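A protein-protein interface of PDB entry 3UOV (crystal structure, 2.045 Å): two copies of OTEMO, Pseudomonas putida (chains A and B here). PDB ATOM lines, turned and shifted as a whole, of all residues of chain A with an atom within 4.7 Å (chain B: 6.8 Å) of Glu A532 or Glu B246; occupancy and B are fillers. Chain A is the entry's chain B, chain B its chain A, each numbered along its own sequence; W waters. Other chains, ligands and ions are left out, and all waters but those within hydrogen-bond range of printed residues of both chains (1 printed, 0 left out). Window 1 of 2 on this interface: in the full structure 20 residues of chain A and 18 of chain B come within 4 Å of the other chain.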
ATOM      1  N   TRP A 456      18.195  21.653   3.251  1.00  0.00           N
ATOM      2  CA  TRP A 456      19.422  22.385   3.624  1.00  0.00           C
ATOM      3  C   TRP A 456      19.815  22.083   5.074  1.00  0.00           C
ATOM      4  O   TRP A 456      20.995  21.831   5.373  1.00  0.00           O
ATOM      5  CB  TRP A 456      19.260  23.909   3.411  1.00  0.00           C
ATOM      6  CG  TRP A 456      20.578  24.672   3.567  1.00  0.00           C
ATOM      7  CD1 TRP A 456      21.496  24.945   2.577  1.00  0.00           C
ATOM      8  CD2 TRP A 456      21.141  25.180   4.789  1.00  0.00           C
ATOM      9  NE1 TRP A 456      22.580  25.614   3.115  1.00  0.00           N
ATOM     10  CE2 TRP A 456      22.392  25.756   4.469  1.00  0.00           C
ATOM     11  CE3 TRP A 456      20.712  25.193   6.129  1.00  0.00           C
ATOM     12  CZ2 TRP A 456      23.197  26.368   5.426  1.00  0.00           C
ATOM     13  CZ3 TRP A 456      21.522  25.791   7.090  1.00  0.00           C
ATOM     14  CH2 TRP A 456      22.755  26.377   6.729  1.00  0.00           C
ATOM     15  N   ARG A 459      21.199  18.688   5.568  1.00  0.00           N
ATOM     16  CA  ARG A 459      22.606  18.683   5.142  1.00  0.00           C
ATOM     17  C   ARG A 459      23.541  19.273   6.205  1.00  0.00           C
ATOM     18  O   ARG A 459      24.616  18.734   6.455  1.00  0.00           O
ATOM     19  CB  ARG A 459      22.770  19.376   3.790  1.00  0.00           C
ATOM     20  CG  ARG A 459      22.236  18.557   2.623  1.00  0.00           C
ATOM     21  CD  ARG A 459      22.640  19.158   1.274  1.00  0.00           C
ATOM     22  NE  ARG A 459      22.050  20.464   1.008  1.00  0.00           N
ATOM     23  CZ  ARG A 459      20.876  20.665   0.413  1.00  0.00           C
ATOM     24  NH1 ARG A 459      20.451  21.896   0.182  1.00  0.00           N
ATOM     25  NH2 ARG A 459      20.131  19.652   0.027  1.00  0.00           N
ATOM     26  N   ARG A 528      18.824  30.923  -1.461  1.00  0.00           N
ATOM     27  CA  ARG A 528      19.384  29.590  -1.370  1.00  0.00           C
ATOM     28  C   ARG A 528      20.828  29.527  -1.847  1.00  0.00           C
ATOM     29  O   ARG A 528      21.636  28.782  -1.292  1.00  0.00           O
ATOM     30  CB  ARG A 528      18.487  28.591  -2.088  1.00  0.00           C
ATOM     31  CG  ARG A 528      17.139  28.459  -1.373  1.00  0.00           C
ATOM     32  CD  ARG A 528      16.335  27.319  -1.899  1.00  0.00           C
ATOM     33  NE  ARG A 528      15.933  27.526  -3.286  1.00  0.00           N
ATOM     34  CZ  ARG A 528      14.811  28.141  -3.655  1.00  0.00           C
ATOM     35  NH1 ARG A 528      13.979  28.628  -2.728  1.00  0.00           N
ATOM     36  NH2 ARG A 528      14.525  28.269  -4.951  1.00  0.00           N
ATOM     37  N   LYS A 529      21.154  30.317  -2.862  1.00  0.00           N
ATOM     38  CA  LYS A 529      22.553  30.484  -3.296  1.00  0.00           C
ATOM     39  C   LYS A 529      23.427  30.947  -2.114  1.00  0.00           C
ATOM     40  O   LYS A 529      24.516  30.402  -1.874  1.00  0.00           O
ATOM     41  CB  LYS A 529      22.620  31.497  -4.430  1.00  0.00           C
ATOM     42  CG  LYS A 529      24.012  31.800  -4.941  1.00  0.00           C
ATOM     43  CD  LYS A 529      23.967  32.905  -6.016  1.00  0.00           C
ATOM     44  CE  LYS A 529      24.276  34.268  -5.395  1.00  0.00           C
ATOM     45  NZ  LYS A 529      23.930  35.466  -6.255  1.00  0.00           N
ATOM     46  N   ARG A 530      22.937  31.933  -1.365  1.00  0.00           N
ATOM     47  CA  ARG A 530      23.642  32.405  -0.180  1.00  0.00           C
ATOM     48  C   ARG A 530      23.844  31.285   0.825  1.00  0.00           C
ATOM     49  O   ARG A 530      24.915  31.156   1.401  1.00  0.00           O
ATOM     50  CB  ARG A 530      22.908  33.594   0.463  1.00  0.00           C
ATOM     51  CG  ARG A 530      23.028  34.896  -0.356  1.00  0.00           C
ATOM     52  CD  ARG A 530      24.434  35.544  -0.218  1.00  0.00           C
ATOM     53  NE  ARG A 530      24.753  35.930   1.168  1.00  0.00           N
ATOM     54  CZ  ARG A 530      25.579  35.262   1.986  1.00  0.00           C
ATOM     55  NH1 ARG A 530      25.789  35.705   3.231  1.00  0.00           N
ATOM     56  NH2 ARG A 530      26.206  34.159   1.574  1.00  0.00           N
ATOM     57  N   CYS A 531      22.803  30.489   1.047  1.00  0.00           N
ATOM     58  CA  CYS A 531      22.887  29.356   1.973  1.00  0.00           C
ATOM     59  C   CYS A 531      23.936  28.328   1.537  1.00  0.00           C
ATOM     60  O   CYS A 531      24.681  27.821   2.362  1.00  0.00           O
ATOM     61  CB  CYS A 531      21.507  28.705   2.125  1.00  0.00           C
ATOM     62  SG  CYS A 531      20.340  29.797   2.978  1.00  0.00           S
ATOM     63  N   GLU A 532      23.987  28.015   0.247  1.00  0.00           N
ATOM     64  CA  GLU A 532      25.008  27.084  -0.268  1.00  0.00           C
ATOM     65  C   GLU A 532      26.438  27.630  -0.220  1.00  0.00           C
ATOM     66  O   GLU A 532      27.384  26.857   0.007  1.00  0.00           O
ATOM     67  CB  GLU A 532      24.661  26.561  -1.675  1.00  0.00           C
ATOM     68  CG  GLU A 532      23.325  25.829  -1.764  1.00  0.00           C
ATOM     69  CD  GLU A 532      23.164  24.635  -0.784  1.00  0.00           C
ATOM     70  OE1 GLU A 532      22.040  24.107  -0.692  1.00  0.00           O
ATOM     71  OE2 GLU A 532      24.130  24.214  -0.126  1.00  0.00           O
ATOM     72  N   GLN A 533      26.603  28.946  -0.422  1.00  0.00           N
ATOM     73  CA  GLN A 533      27.923  29.582  -0.249  1.00  0.00           C
ATOM     74  C   GLN A 533      28.437  29.328   1.179  1.00  0.00           C
ATOM     75  O   GLN A 533      29.601  28.946   1.395  1.00  0.00           O
ATOM     76  CB  GLN A 533      27.851  31.093  -0.560  1.00  0.00           C
ATOM     77  CG  GLN A 533      27.493  31.424  -2.022  1.00  0.00           C
ATOM     78  CD  GLN A 533      27.374  32.930  -2.318  1.00  0.00           C
ATOM     79  OE1 GLN A 533      27.342  33.768  -1.409  1.00  0.00           O
ATOM     80  NE2 GLN A 533      27.326  33.271  -3.604  1.00  0.00           N
ATOM     81  N   VAL A 534      27.538  29.500   2.153  1.00  0.00           N
ATOM     82  CA  VAL A 534      27.853  29.268   3.570  1.00  0.00           C
ATOM     83  C   VAL A 534      28.125  27.789   3.840  1.00  0.00           C
ATOM     84  O   VAL A 534      29.160  27.452   4.383  1.00  0.00           O
ATOM     85  CB  VAL A 534      26.737  29.828   4.502  1.00  0.00           C
ATOM     86  CG1 VAL A 534      26.934  29.395   5.938  1.00  0.00           C
ATOM     87  CG2 VAL A 534      26.700  31.386   4.422  1.00  0.00           C
ATOM     88  N   ALA A 535      27.212  26.911   3.437  1.00  0.00           N
ATOM     89  CA  ALA A 535      27.374  25.485   3.702  1.00  0.00           C
ATOM     90  C   ALA A 535      28.687  24.944   3.128  1.00  0.00           C
ATOM     91  O   ALA A 535      29.435  24.239   3.821  1.00  0.00           O
ATOM     92  CB  ALA A 535      26.177  24.702   3.169  1.00  0.00           C
ATOM     93  N   TYR A 536      28.967  25.266   1.863  1.00  0.00           N
ATOM     94  CA  TYR A 536      30.186  24.766   1.219  1.00  0.00           C
ATOM     95  C   TYR A 536      31.433  25.195   1.976  1.00  0.00           C
ATOM     96  O   TYR A 536      32.364  24.404   2.148  1.00  0.00           O
ATOM     97  CB  TYR A 536      30.299  25.232  -0.240  1.00  0.00           C
ATOM     98  CG  TYR A 536      31.628  24.863  -0.856  1.00  0.00           C
ATOM     99  CD1 TYR A 536      31.854  23.578  -1.335  1.00  0.00           C
ATOM    100  CD2 TYR A 536      32.669  25.793  -0.933  1.00  0.00           C
ATOM    101  CE1 TYR A 536      33.083  23.223  -1.890  1.00  0.00           C
ATOM    102  CE2 TYR A 536      33.908  25.452  -1.497  1.00  0.00           C
ATOM    103  CZ  TYR A 536      34.101  24.174  -1.964  1.00  0.00           C
ATOM    104  OH  TYR A 536      35.303  23.828  -2.513  1.00  0.00           O
ATOM    105  N   TYR B 241      29.229  15.585  -0.671  1.00  0.00           N
ATOM    106  CA  TYR B 241      28.830  15.673  -2.075  1.00  0.00           C
ATOM    107  C   TYR B 241      27.490  16.397  -2.293  1.00  0.00           C
ATOM    108  O   TYR B 241      27.412  17.250  -3.187  1.00  0.00           O
ATOM    109  CB  TYR B 241      28.813  14.291  -2.762  1.00  0.00           C
ATOM    110  CG  TYR B 241      30.132  13.856  -3.388  1.00  0.00           C
ATOM    111  CD1 TYR B 241      31.261  14.689  -3.379  1.00  0.00           C
ATOM    112  CD2 TYR B 241      30.229  12.620  -4.032  1.00  0.00           C
ATOM    113  CE1 TYR B 241      32.451  14.286  -3.961  1.00  0.00           C
ATOM    114  CE2 TYR B 241      31.419  12.215  -4.643  1.00  0.00           C
ATOM    115  CZ  TYR B 241      32.521  13.044  -4.601  1.00  0.00           C
ATOM    116  OH  TYR B 241      33.690  12.631  -5.208  1.00  0.00           O
ATOM    117  N   PRO B 242      26.441  16.080  -1.481  1.00  0.00           N
ATOM    118  CA  PRO B 242      25.151  16.789  -1.659  1.00  0.00           C
ATOM    119  C   PRO B 242      25.225  18.318  -1.581  1.00  0.00           C
ATOM    120  O   PRO B 242      24.565  18.993  -2.360  1.00  0.00           O
ATOM    121  CB  PRO B 242      24.270  16.206  -0.548  1.00  0.00           C
ATOM    122  CG  PRO B 242      24.837  14.812  -0.344  1.00  0.00           C
ATOM    123  CD  PRO B 242      26.329  15.057  -0.420  1.00  0.00           C
ATOM    124  N   THR B 243      26.026  18.844  -0.663  1.00  0.00           N
ATOM    125  CA  THR B 243      26.278  20.274  -0.552  1.00  0.00           C
ATOM    126  C   THR B 243      27.145  20.760  -1.710  1.00  0.00           C
ATOM    127  O   THR B 243      26.869  21.820  -2.284  1.00  0.00           O
ATOM    128  CB  THR B 243      26.982  20.606   0.776  1.00  0.00           C
ATOM    129  OG1 THR B 243      26.058  20.429   1.855  1.00  0.00           O
ATOM    130  CG2 THR B 243      27.501  22.050   0.777  1.00  0.00           C
ATOM    131  N   ILE B 244      28.190  19.999  -2.042  1.00  0.00           N
ATOM    132  CA  ILE B 244      29.108  20.371  -3.145  1.00  0.00           C
ATOM    133  C   ILE B 244      28.349  20.535  -4.471  1.00  0.00           C
ATOM    134  O   ILE B 244      28.510  21.526  -5.167  1.00  0.00           O
ATOM    135  CB  ILE B 244      30.285  19.373  -3.282  1.00  0.00           C
ATOM    136  CG1 ILE B 244      31.208  19.518  -2.061  1.00  0.00           C
ATOM    137  CG2 ILE B 244      31.081  19.621  -4.582  1.00  0.00           C
ATOM    138  CD1 ILE B 244      32.183  18.361  -1.863  1.00  0.00           C
ATOM    139  N   LEU B 245      27.511  19.559  -4.783  1.00  0.00           N
ATOM    140  CA  LEU B 245      26.647  19.605  -5.953  1.00  0.00           C
ATOM    141  C   LEU B 245      25.737  20.838  -5.969  1.00  0.00           C
ATOM    142  O   LEU B 245      25.635  21.541  -6.977  1.00  0.00           O
ATOM    143  CB  LEU B 245      25.817  18.306  -5.999  1.00  0.00           C
ATOM    144  CG  LEU B 245      24.909  18.096  -7.198  1.00  0.00           C
ATOM    145  CD1 LEU B 245      25.683  18.167  -8.520  1.00  0.00           C
ATOM    146  CD2 LEU B 245      24.140  16.769  -7.046  1.00  0.00           C
ATOM    147  N   GLU B 246      25.070  21.112  -4.850  1.00  0.00           N
ATOM    148  CA  GLU B 246      24.180  22.272  -4.796  1.00  0.00           C
ATOM    149  C   GLU B 246      24.975  23.561  -4.945  1.00  0.00           C
ATOM    150  O   GLU B 246      24.509  24.511  -5.565  1.00  0.00           O
ATOM    151  CB  GLU B 246      23.327  22.289  -3.506  1.00  0.00           C
ATOM    152  CG  GLU B 246      22.323  21.111  -3.390  1.00  0.00           C
ATOM    153  CD  GLU B 246      21.386  20.984  -4.598  1.00  0.00           C
ATOM    154  OE1 GLU B 246      20.738  21.982  -4.954  1.00  0.00           O
ATOM    155  OE2 GLU B 246      21.293  19.885  -5.195  1.00  0.00           O
ATOM    156  N   TYR B 247      26.175  23.589  -4.389  1.00  0.00           N
ATOM    157  CA  TYR B 247      27.039  24.765  -4.525  1.00  0.00           C
ATOM    158  C   TYR B 247      27.504  25.004  -5.972  1.00  0.00           C
ATOM    159  O   TYR B 247      27.422  26.129  -6.470  1.00  0.00           O
ATOM    160  CB  TYR B 247      28.258  24.649  -3.612  1.00  0.00           C
ATOM    161  CG  TYR B 247      29.203  25.826  -3.677  1.00  0.00           C
ATOM    162  CD1 TYR B 247      28.747  27.124  -3.438  1.00  0.00           C
ATOM    163  CD2 TYR B 247      30.557  25.643  -3.958  1.00  0.00           C
ATOM    164  CE1 TYR B 247      29.606  28.214  -3.484  1.00  0.00           C
ATOM    165  CE2 TYR B 247      31.435  26.742  -4.002  1.00  0.00           C
ATOM    166  CZ  TYR B 247      30.951  28.015  -3.761  1.00  0.00           C
ATOM    167  OH  TYR B 247      31.803  29.112  -3.790  1.00  0.00           O
ATOM    168  N   VAL B 248      28.012  23.970  -6.641  1.00  0.00           N
ATOM    169  CA  VAL B 248      28.535  24.174  -8.013  1.00  0.00           C
ATOM    170  C   VAL B 248      27.422  24.457  -9.034  1.00  0.00           C
ATOM    171  O   VAL B 248      27.665  25.126 -10.053  1.00  0.00           O
ATOM    172  CB  VAL B 248      29.458  23.015  -8.495  1.00  0.00           C
ATOM    173  CG1 VAL B 248      30.744  22.918  -7.626  1.00  0.00           C
ATOM    174  CG2 VAL B 248      28.709  21.688  -8.512  1.00  0.00           C
ATOM    175  N   LYS B 249      26.213  23.956  -8.759  1.00  0.00           N
ATOM    176  CA  LYS B 249      25.012  24.333  -9.517  1.00  0.00           C
ATOM    177  C   LYS B 249      24.582  25.800  -9.346  1.00  0.00           C
ATOM    178  O   LYS B 249      23.732  26.282 -10.106  1.00  0.00           O
ATOM    179  CB  LYS B 249      23.839  23.398  -9.193  1.00  0.00           C
ATOM    180  CG  LYS B 249      24.042  21.963  -9.719  1.00  0.00           C
ATOM    181  CD  LYS B 249      22.910  20.984  -9.312  1.00  0.00           C
ATOM    182  CE  LYS B 249      21.582  21.336  -9.982  1.00  0.00           C
ATOM    183  NZ  LYS B 249      20.707  20.128 -10.116  1.00  0.00           N
ATOM    184  N   SER B 250      25.170  26.498  -8.373  1.00  0.00           N
ATOM    185  CA  SER B 250      24.705  27.827  -7.964  1.00  0.00           C
ATOM    186  C   SER B 250      25.732  28.931  -8.217  1.00  0.00           C
ATOM    187  O   SER B 250      25.419  30.114  -8.049  1.00  0.00           O
ATOM    188  CB  SER B 250      24.336  27.824  -6.465  1.00  0.00           C
ATOM    189  OG  SER B 250      25.451  28.235  -5.684  1.00  0.00           O
ATOM    190  N   THR B 251      26.953  28.555  -8.605  1.00  0.00           N
ATOM    191  CA  THR B 251      27.999  29.541  -8.875  1.00  0.00           C
ATOM    192  C   THR B 251      27.927  29.898 -10.338  1.00  0.00           C
ATOM    193  O   THR B 251      27.377  29.154 -11.141  1.00  0.00           O
ATOM    194  CB  THR B 251      29.437  29.034  -8.519  1.00  0.00           C
ATOM    195  OG1 THR B 251      29.821  27.971  -9.405  1.00  0.00           O
ATOM    196  CG2 THR B 251      29.509  28.545  -7.071  1.00  0.00           C
ATOM    197  N   HIS B 258      32.942  31.668  -5.791  1.00  0.00           N
ATOM    198  CA  HIS B 258      32.059  32.785  -6.094  1.00  0.00           C
ATOM    199  C   HIS B 258      32.737  34.097  -5.715  1.00  0.00           C
ATOM    200  O   HIS B 258      33.565  34.149  -4.801  1.00  0.00           O
ATOM    201  CB  HIS B 258      30.747  32.643  -5.337  1.00  0.00           C
ATOM    202  CG  HIS B 258      30.905  32.666  -3.854  1.00  0.00           C
ATOM    203  ND1 HIS B 258      31.231  31.544  -3.123  1.00  0.00           N
ATOM    204  CD2 HIS B 258      30.790  33.679  -2.964  1.00  0.00           C
ATOM    205  CE1 HIS B 258      31.310  31.866  -1.843  1.00  0.00           C
ATOM    206  NE2 HIS B 258      31.055  33.157  -1.722  1.00  0.00           N
HETATM  207  O   HOH W   1      23.942  22.476   1.916  1.00  0.00           O
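No position is printed for both chains. Of the 10 pairs that touch across the chains among the printed residues, none has its exchanged pair printed and touching as well.
Water W1 lies within hydrogen-bond range of OE2 of Glu A532 (2.7 Å), NE of Arg A459 (2.9 Å) and OG1 of Thr B243 (2.9 Å).
The side-chain hydroxyl of Ser B250 lies within hydrogen-bond range of the backbone carbonyl oxygen of Tyr B247 (3.0 Å). The guanidinium group of Arg A459 is in salt-bridge range of the side-chain carboxylate of Glu A532, at 2.9 Å. ND1 of His B258 is in hydrogen-bond range of OH of Tyr B247 (2.6 Å). The guanidinium group (NH2) of Arg A530 lies within hydrogen-bond range of the side-chain amide oxygen (OE1) of Gln A533.
Of the 11 printed residues of chain A, 6 touch a printed residue of chain B. Hydrophobic or aromatic side chains of chain A that line the printed part of chain B: Ala A535 and Tyr A536. Printed residues of chain B that touch a printed residue of chain A: Pro B242, Thr B243, Glu B246, Tyr B247, Ser B250 and His B258. Along chain B the printed residues that touch a printed residue of chain A span positions 242 to 258. Among the printed residues, 10 pairs touch across the chains. Among the printed residues, no Asp or Glu carboxylate lies within 4 Å of a Lys or Arg side-chain nitrogen of the other chain.
Printed residues of chain B within 4 Å of Arg A459: Pro B242 (3.8 Å) and Thr B243 (3.7 Å). Of the printed residues of chain B, Lys A529 touches Ser B250 (3.7 Å). Cys A531 touches none of the printed residues of chain B. Of chain B, only Glu B246 and Tyr B247 come within 4 Å of Glu A532. Tyr B241 touches none of the printed residues of chain A. Glu B246 touches one residue of chain A. Of the printed residues of chain A, Tyr B247 touches Glu A532, Gln A533 and Tyr A536. The nearest residue of chain B that does not touch Glu A532 is Thr B243 (4.1 Å). The nearest printed residue of chain A that does not touch Ser B250 is Glu A532 (4.4 Å).
CD of Arg A459 touches CB of Pro B242 (3.8 Å). OG1 of Thr B243 touches CD of Arg A459 (3.7 Å). Lys A529 touches Ser B250. Glu B246 touches Glu A532 (CB to OE1, 3.6 Å). O of Glu A532 touches CD1 of Tyr B247, at 3.7 Å. CE1 of Tyr B247 touches CA of Gln A533 (3.9 Å). Gln A533 touches His B258 (NE2 to CD2, 3.5 Å). Ala A535 touches Thr B243. N of Tyr A536 touches CG2 of Thr B243 (3.7 Å). Tyr A536 touches Tyr B247.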
